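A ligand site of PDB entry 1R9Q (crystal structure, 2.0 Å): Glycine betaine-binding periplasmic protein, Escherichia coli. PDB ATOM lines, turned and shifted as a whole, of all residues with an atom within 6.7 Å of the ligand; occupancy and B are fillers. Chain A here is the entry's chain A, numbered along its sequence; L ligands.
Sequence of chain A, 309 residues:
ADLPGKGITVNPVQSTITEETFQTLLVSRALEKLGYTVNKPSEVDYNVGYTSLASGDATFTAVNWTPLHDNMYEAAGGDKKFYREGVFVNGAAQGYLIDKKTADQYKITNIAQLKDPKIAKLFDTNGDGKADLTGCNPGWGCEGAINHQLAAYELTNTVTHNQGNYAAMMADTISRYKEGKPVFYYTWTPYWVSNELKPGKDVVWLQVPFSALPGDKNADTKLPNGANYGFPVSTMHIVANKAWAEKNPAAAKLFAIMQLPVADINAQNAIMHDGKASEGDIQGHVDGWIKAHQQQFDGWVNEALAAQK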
ATOM      1  N   SER A  15      17.855  12.406   5.288  1.00  0.00           N
ATOM      2  CA  SER A  15      17.859  13.386   4.204  1.00  0.00           C
ATOM      3  C   SER A  15      18.273  12.743   2.887  1.00  0.00           C
ATOM      4  O   SER A  15      18.464  11.523   2.814  1.00  0.00           O
ATOM      5  CB  SER A  15      18.723  14.608   4.543  1.00  0.00           C
ATOM      6  OG  SER A  15      20.105  14.340   4.420  1.00  0.00           O
ATOM      7  N   ILE A  17      21.107  13.228   1.635  1.00  0.00           N
ATOM      8  CA  ILE A  17      22.515  12.925   1.814  1.00  0.00           C
ATOM      9  C   ILE A  17      22.714  11.418   1.957  1.00  0.00           C
ATOM     10  O   ILE A  17      22.409  10.834   3.005  1.00  0.00           O
ATOM     11  CB  ILE A  17      23.058  13.644   3.090  1.00  0.00           C
ATOM     12  CG1 ILE A  17      22.965  15.174   2.929  1.00  0.00           C
ATOM     13  CG2 ILE A  17      24.496  13.225   3.361  1.00  0.00           C
ATOM     14  CD1 ILE A  17      23.276  15.941   4.227  1.00  0.00           C
ATOM     15  N   GLU A  20      24.226   9.402   4.906  1.00  0.00           N
ATOM     16  CA  GLU A  20      23.410   9.142   6.089  1.00  0.00           C
ATOM     17  C   GLU A  20      22.786   7.734   6.111  1.00  0.00           C
ATOM     18  O   GLU A  20      22.243   7.302   7.142  1.00  0.00           O
ATOM     19  CB  GLU A  20      22.302  10.186   6.167  1.00  0.00           C
ATOM     20  CG  GLU A  20      22.816  11.532   6.590  1.00  0.00           C
ATOM     21  CD  GLU A  20      21.754  12.595   6.742  1.00  0.00           C
ATOM     22  OE1 GLU A  20      20.607  12.455   6.263  1.00  0.00           O
ATOM     23  OE2 GLU A  20      22.095  13.608   7.383  1.00  0.00           O
ATOM     24  N   TYR A  46      15.231  17.805   5.767  1.00  0.00           N
ATOM     25  CA  TYR A  46      15.199  17.604   7.226  1.00  0.00           C
ATOM     26  C   TYR A  46      13.892  18.099   7.830  1.00  0.00           C
ATOM     27  O   TYR A  46      13.272  17.404   8.626  1.00  0.00           O
ATOM     28  CB  TYR A  46      16.356  18.331   7.902  1.00  0.00           C
ATOM     29  CG  TYR A  46      17.732  17.711   7.699  1.00  0.00           C
ATOM     30  CD1 TYR A  46      18.770  18.446   7.126  1.00  0.00           C
ATOM     31  CD2 TYR A  46      17.993  16.383   8.083  1.00  0.00           C
ATOM     32  CE1 TYR A  46      20.030  17.895   6.947  1.00  0.00           C
ATOM     33  CE2 TYR A  46      19.284  15.826   7.899  1.00  0.00           C
ATOM     34  CZ  TYR A  46      20.290  16.591   7.335  1.00  0.00           C
ATOM     35  OH  TYR A  46      21.558  16.070   7.151  1.00  0.00           O
ATOM     36  N   VAL A  63      19.522  10.848  12.257  1.00  0.00           N
ATOM     37  CA  VAL A  63      20.395  11.946  11.863  1.00  0.00           C
ATOM     38  C   VAL A  63      19.947  13.286  12.469  1.00  0.00           C
ATOM     39  O   VAL A  63      20.058  14.330  11.860  1.00  0.00           O
ATOM     40  CB  VAL A  63      20.490  12.046  10.302  1.00  0.00           C
ATOM     41  CG1 VAL A  63      21.152  10.795   9.745  1.00  0.00           C
ATOM     42  CG2 VAL A  63      19.101  12.247   9.666  1.00  0.00           C
ATOM     43  N   TRP A  65      20.726  16.250  14.457  1.00  0.00           N
ATOM     44  CA  TRP A  65      21.933  16.918  14.908  1.00  0.00           C
ATOM     45  C   TRP A  65      21.638  17.943  16.025  1.00  0.00           C
ATOM     46  O   TRP A  65      20.640  18.682  15.962  1.00  0.00           O
ATOM     47  CB  TRP A  65      22.571  17.667  13.745  1.00  0.00           C
ATOM     48  CG  TRP A  65      23.373  16.838  12.778  1.00  0.00           C
ATOM     49  CD1 TRP A  65      22.900  16.035  11.783  1.00  0.00           C
ATOM     50  CD2 TRP A  65      24.802  16.781  12.688  1.00  0.00           C
ATOM     51  NE1 TRP A  65      23.940  15.467  11.084  1.00  0.00           N
ATOM     52  CE2 TRP A  65      25.121  15.911  11.619  1.00  0.00           C
ATOM     53  CE3 TRP A  65      25.848  17.365  13.411  1.00  0.00           C
ATOM     54  CZ2 TRP A  65      26.443  15.616  11.267  1.00  0.00           C
ATOM     55  CZ3 TRP A  65      27.150  17.090  13.051  1.00  0.00           C
ATOM     56  CH2 TRP A  65      27.426  16.211  11.976  1.00  0.00           C
ATOM     57  N   LEU A  68      22.605  21.958  15.536  1.00  0.00           N
ATOM     58  CA  LEU A  68      22.192  22.491  14.243  1.00  0.00           C
ATOM     59  C   LEU A  68      20.718  22.289  13.908  1.00  0.00           C
ATOM     60  O   LEU A  68      20.178  23.057  13.114  1.00  0.00           O
ATOM     61  CB  LEU A  68      23.041  21.899  13.108  1.00  0.00           C
ATOM     62  CG  LEU A  68      24.405  22.535  12.841  1.00  0.00           C
ATOM     63  CD1 LEU A  68      24.962  22.055  11.525  1.00  0.00           C
ATOM     64  CD2 LEU A  68      24.346  24.052  12.866  1.00  0.00           C
ATOM     65  N   HIS A  69      20.084  21.263  14.480  1.00  0.00           N
ATOM     66  CA  HIS A  69      18.667  20.980  14.243  1.00  0.00           C
ATOM     67  C   HIS A  69      17.717  21.493  15.377  1.00  0.00           C
ATOM     68  O   HIS A  69      16.519  21.310  15.281  1.00  0.00           O
ATOM     69  CB  HIS A  69      18.456  19.471  14.013  1.00  0.00           C
ATOM     70  CG  HIS A  69      19.025  18.973  12.710  1.00  0.00           C
ATOM     71  ND1 HIS A  69      18.468  17.919  12.004  1.00  0.00           N
ATOM     72  CD2 HIS A  69      20.085  19.391  11.972  1.00  0.00           C
ATOM     73  CE1 HIS A  69      19.146  17.728  10.895  1.00  0.00           C
ATOM     74  NE2 HIS A  69      20.127  18.600  10.841  1.00  0.00           N
ATOM     75  N   MET A  72      14.637  23.445  14.257  1.00  0.00           N
ATOM     76  CA  MET A  72      13.636  22.647  13.542  1.00  0.00           C
ATOM     77  C   MET A  72      12.951  21.663  14.463  1.00  0.00           C
ATOM     78  O   MET A  72      11.777  21.354  14.275  1.00  0.00           O
ATOM     79  CB  MET A  72      14.271  21.840  12.398  1.00  0.00           C
ATOM     80  CG  MET A  72      14.627  22.640  11.162  1.00  0.00           C
ATOM     81  SD  MET A  72      15.373  21.545   9.935  1.00  0.00           S
ATOM     82  CE  MET A  72      17.026  21.607  10.436  1.00  0.00           C
ATOM     83  N   GLN A  94      32.646  20.509  12.983  1.00  0.00           N
ATOM     84  CA  GLN A  94      32.321  21.295  11.794  1.00  0.00           C
ATOM     85  C   GLN A  94      33.012  22.660  11.885  1.00  0.00           C
ATOM     86  O   GLN A  94      33.549  23.036  12.936  1.00  0.00           O
ATOM     87  CB  GLN A  94      30.795  21.459  11.624  1.00  0.00           C
ATOM     88  CG  GLN A  94      30.095  21.876  12.870  1.00  0.00           C
ATOM     89  CD  GLN A  94      28.581  21.823  12.808  1.00  0.00           C
ATOM     90  OE1 GLN A  94      27.938  21.413  13.770  1.00  0.00           O
ATOM     91  NE2 GLN A  94      28.004  22.303  11.736  1.00  0.00           N
ATOM     92  N   CYS A 136      26.182  25.631   2.469  1.00  0.00           N
ATOM     93  CA  CYS A 136      25.181  24.613   2.700  1.00  0.00           C
ATOM     94  C   CYS A 136      23.941  24.733   1.817  1.00  0.00           C
ATOM     95  O   CYS A 136      23.558  25.828   1.408  1.00  0.00           O
ATOM     96  CB  CYS A 136      24.772  24.669   4.166  1.00  0.00           C
ATOM     97  SG  CYS A 136      26.100  24.244   5.292  1.00  0.00           S
ATOM     98  N   GLY A 139      17.761  24.466   3.422  1.00  0.00           N
ATOM     99  CA  GLY A 139      17.134  23.492   4.287  1.00  0.00           C
ATOM    100  C   GLY A 139      18.051  22.806   5.289  1.00  0.00           C
ATOM    101  O   GLY A 139      17.574  22.250   6.263  1.00  0.00           O
ATOM    102  N   TRP A 140      19.360  22.819   5.061  1.00  0.00           N
ATOM    103  CA  TRP A 140      20.313  22.280   6.029  1.00  0.00           C
ATOM    104  C   TRP A 140      20.393  23.212   7.224  1.00  0.00           C
ATOM    105  O   TRP A 140      20.272  24.426   7.072  1.00  0.00           O
ATOM    106  CB  TRP A 140      21.687  22.092   5.405  1.00  0.00           C
ATOM    107  CG  TRP A 140      21.750  20.982   4.404  1.00  0.00           C
ATOM    108  CD1 TRP A 140      20.731  20.180   3.996  1.00  0.00           C
ATOM    109  CD2 TRP A 140      22.914  20.524   3.729  1.00  0.00           C
ATOM    110  NE1 TRP A 140      21.182  19.275   3.069  1.00  0.00           N
ATOM    111  CE2 TRP A 140      22.521  19.454   2.892  1.00  0.00           C
ATOM    112  CE3 TRP A 140      24.259  20.930   3.721  1.00  0.00           C
ATOM    113  CZ2 TRP A 140      23.414  18.780   2.080  1.00  0.00           C
ATOM    114  CZ3 TRP A 140      25.155  20.241   2.901  1.00  0.00           C
ATOM    115  CH2 TRP A 140      24.720  19.187   2.087  1.00  0.00           C
ATOM    116  N   GLY A 141      20.579  22.639   8.407  1.00  0.00           N
ATOM    117  CA  GLY A 141      20.767  23.397   9.613  1.00  0.00           C
ATOM    118  C   GLY A 141      21.946  24.342   9.547  1.00  0.00           C
ATOM    119  O   GLY A 141      21.892  25.444  10.099  1.00  0.00           O
ATOM    120  N   CYS A 142      22.990  23.951   8.823  1.00  0.00           N
ATOM    121  CA  CYS A 142      24.172  24.798   8.694  1.00  0.00           C
ATOM    122  C   CYS A 142      23.930  26.008   7.796  1.00  0.00           C
ATOM    123  O   CYS A 142      24.672  26.972   7.878  1.00  0.00           O
ATOM    124  CB  CYS A 142      25.383  23.986   8.221  1.00  0.00           C
ATOM    125  SG  CYS A 142      25.170  23.090   6.680  1.00  0.00           S
ATOM    126  N   GLU A 143      22.909  25.964   6.948  1.00  0.00           N
ATOM    127  CA  GLU A 143      22.500  27.153   6.198  1.00  0.00           C
ATOM    128  C   GLU A 143      22.269  28.301   7.170  1.00  0.00           C
ATOM    129  O   GLU A 143      22.842  29.370   7.017  1.00  0.00           O
ATOM    130  CB  GLU A 143      21.227  26.928   5.380  1.00  0.00           C
ATOM    131  CG  GLU A 143      20.618  28.217   4.813  1.00  0.00           C
ATOM    132  CD  GLU A 143      19.389  27.970   3.960  1.00  0.00           C
ATOM    133  OE1 GLU A 143      18.491  27.213   4.383  1.00  0.00           O
ATOM    134  OE2 GLU A 143      19.323  28.500   2.854  1.00  0.00           O
ATOM    135  N   TYR A 186      32.994  25.465   4.177  1.00  0.00           N
ATOM    136  CA  TYR A 186      32.510  24.836   5.390  1.00  0.00           C
ATOM    137  C   TYR A 186      32.457  23.325   5.169  1.00  0.00           C
ATOM    138  O   TYR A 186      32.138  22.868   4.068  1.00  0.00           O
ATOM    139  CB  TYR A 186      31.103  25.345   5.725  1.00  0.00           C
ATOM    140  CG  TYR A 186      30.274  24.487   6.667  1.00  0.00           C
ATOM    141  CD1 TYR A 186      30.275  24.738   8.030  1.00  0.00           C
ATOM    142  CD2 TYR A 186      29.472  23.446   6.185  1.00  0.00           C
ATOM    143  CE1 TYR A 186      29.545  23.976   8.891  1.00  0.00           C
ATOM    144  CE2 TYR A 186      28.729  22.651   7.067  1.00  0.00           C
ATOM    145  CZ  TYR A 186      28.768  22.950   8.423  1.00  0.00           C
ATOM    146  OH  TYR A 186      28.061  22.243   9.335  1.00  0.00           O
ATOM    147  N   THR A 187      32.792  22.562   6.202  1.00  0.00           N
ATOM    148  CA  THR A 187      32.502  21.137   6.171  1.00  0.00           C
ATOM    149  C   THR A 187      32.242  20.603   7.563  1.00  0.00           C
ATOM    150  O   THR A 187      32.324  21.322   8.551  1.00  0.00           O
ATOM    151  CB  THR A 187      33.609  20.353   5.412  1.00  0.00           C
ATOM    152  OG1 THR A 187      33.078  19.114   4.906  1.00  0.00           O
ATOM    153  CG2 THR A 187      34.770  19.968   6.330  1.00  0.00           C
ATOM    154  N   TRP A 188      31.854  19.333   7.622  1.00  0.00           N
ATOM    155  CA  TRP A 188      31.633  18.634   8.865  1.00  0.00           C
ATOM    156  C   TRP A 188      32.195  17.219   8.775  1.00  0.00           C
ATOM    157  O   TRP A 188      32.450  16.692   7.684  1.00  0.00           O
ATOM    158  CB  TRP A 188      30.140  18.566   9.190  1.00  0.00           C
ATOM    159  CG  TRP A 188      29.373  17.690   8.208  1.00  0.00           C
ATOM    160  CD1 TRP A 188      28.971  16.402   8.387  1.00  0.00           C
ATOM    161  CD2 TRP A 188      28.917  18.072   6.916  1.00  0.00           C
ATOM    162  NE1 TRP A 188      28.312  15.943   7.274  1.00  0.00           N
ATOM    163  CE2 TRP A 188      28.261  16.963   6.351  1.00  0.00           C
ATOM    164  CE3 TRP A 188      29.019  19.236   6.162  1.00  0.00           C
ATOM    165  CZ2 TRP A 188      27.708  16.986   5.082  1.00  0.00           C
ATOM    166  CZ3 TRP A 188      28.465  19.274   4.901  1.00  0.00           C
ATOM    167  CH2 TRP A 188      27.808  18.148   4.369  1.00  0.00           C
ATOM    168  N   THR A 189      32.357  16.607   9.940  1.00  0.00           N
ATOM    169  CA  THR A 189      32.556  15.175  10.052  1.00  0.00           C
ATOM    170  C   THR A 189      31.363  14.609  10.800  1.00  0.00           C
ATOM    171  O   THR A 189      30.784  15.294  11.637  1.00  0.00           O
ATOM    172  CB  THR A 189      33.849  14.847  10.843  1.00  0.00           C
ATOM    173  OG1 THR A 189      33.757  15.432  12.157  1.00  0.00           O
ATOM    174  CG2 THR A 189      35.059  15.531  10.226  1.00  0.00           C
ATOM    175  N   PRO A 190      30.957  13.387  10.495  1.00  0.00           N
ATOM    176  CA  PRO A 190      31.570  12.550   9.468  1.00  0.00           C
ATOM    177  C   PRO A 190      31.055  12.862   8.067  1.00  0.00           C
ATOM    178  O   PRO A 190      29.856  13.012   7.873  1.00  0.00           O
ATOM    179  CB  PRO A 190      31.130  11.137   9.865  1.00  0.00           C
ATOM    180  CG  PRO A 190      29.828  11.311  10.522  1.00  0.00           C
ATOM    181  CD  PRO A 190      29.820  12.699  11.141  1.00  0.00           C
ATOM    182  N   MET A 236      24.867  13.424  17.120  1.00  0.00           N
ATOM    183  CA  MET A 236      23.637  12.992  16.460  1.00  0.00           C
ATOM    184  C   MET A 236      22.844  12.082  17.373  1.00  0.00           C
ATOM    185  O   MET A 236      23.419  11.361  18.201  1.00  0.00           O
ATOM    186  CB  MET A 236      23.930  12.299  15.130  1.00  0.00           C
ATOM    187  CG  MET A 236      24.493  13.226  14.086  1.00  0.00           C
ATOM    188  SD  MET A 236      24.794  12.439  12.496  1.00  0.00           S
ATOM    189  CE  MET A 236      26.477  12.164  12.657  1.00  0.00           C
HETATM  190  N1  LIG L   1      24.549  18.521   7.763  1.00  0.00           N
HETATM  191  C1  LIG L   1      25.790  19.193   8.138  1.00  0.00           C
HETATM  192  C2  LIG L   1      23.675  19.031   8.770  1.00  0.00           C
HETATM  193  C3  LIG L   1      24.359  18.939  10.068  1.00  0.00           C
HETATM  194  C4  LIG L   1      25.808  19.246   9.649  1.00  0.00           C
HETATM  195  C5  LIG L   1      24.174  18.861   6.382  1.00  0.00           C
HETATM  196  C6  LIG L   1      24.770  17.069   7.817  1.00  0.00           C
HETATM  197  C7  LIG L   1      22.887  20.107   8.667  1.00  0.00           C
HETATM  198  O1  LIG L   1      23.404  21.176   8.361  1.00  0.00           O
HETATM  199  O2  LIG L   1      21.696  20.118   8.947  1.00  0.00           O
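O2 of the ligand is in hydrogen-bond range of N of Gly 141, at 2.8 Å. A ring nitrogen (NE2) of His 69 is in hydrogen-bond range of an oxygen (O2) of the ligand. The backbone NH (N) of Cys 142 is in hydrogen-bond range of an oxygen (O1) of the ligand (2.8 Å).
Residues that only touch the ligand: Trp 140 (3.4 Å), Tyr 46 (3.4 Å), Trp 65 (3.4 Å), Leu 68 (3.5 Å), Trp 188 (3.5 Å), Ile 17 (3.7 Å) and Tyr 186 (3.8 Å). Hydrophobic or aromatic side chains that line the ligand: Ile 17, Tyr 46, Trp 65, Leu 68, His 69, Trp 140 and Trp 188. Of the 22 residues printed, 10 come within 4 Å of the ligand.
NE1 of Trp 65 sits at hydrogen-bond distance from SD of Met 236. The side-chain hydroxyl of Ser 15 sits close to the backbone NH of Ile 17 (3.2 Å). The side-chain hydroxyl (OH) of Tyr 186 is in hydrogen-bond range of the side-chain amide nitrogen (NE2) of Gln 94. OH of Tyr 46 sits at hydrogen-bond distance from OE2 of Glu 20 (2.5 Å). NE1 of Trp 188 lies within hydrogen-bond range of O of Pro 190 (3.4 Å). SG of Cys 142 forms a disulfide with SG of Cys 136 (2.0 Å).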
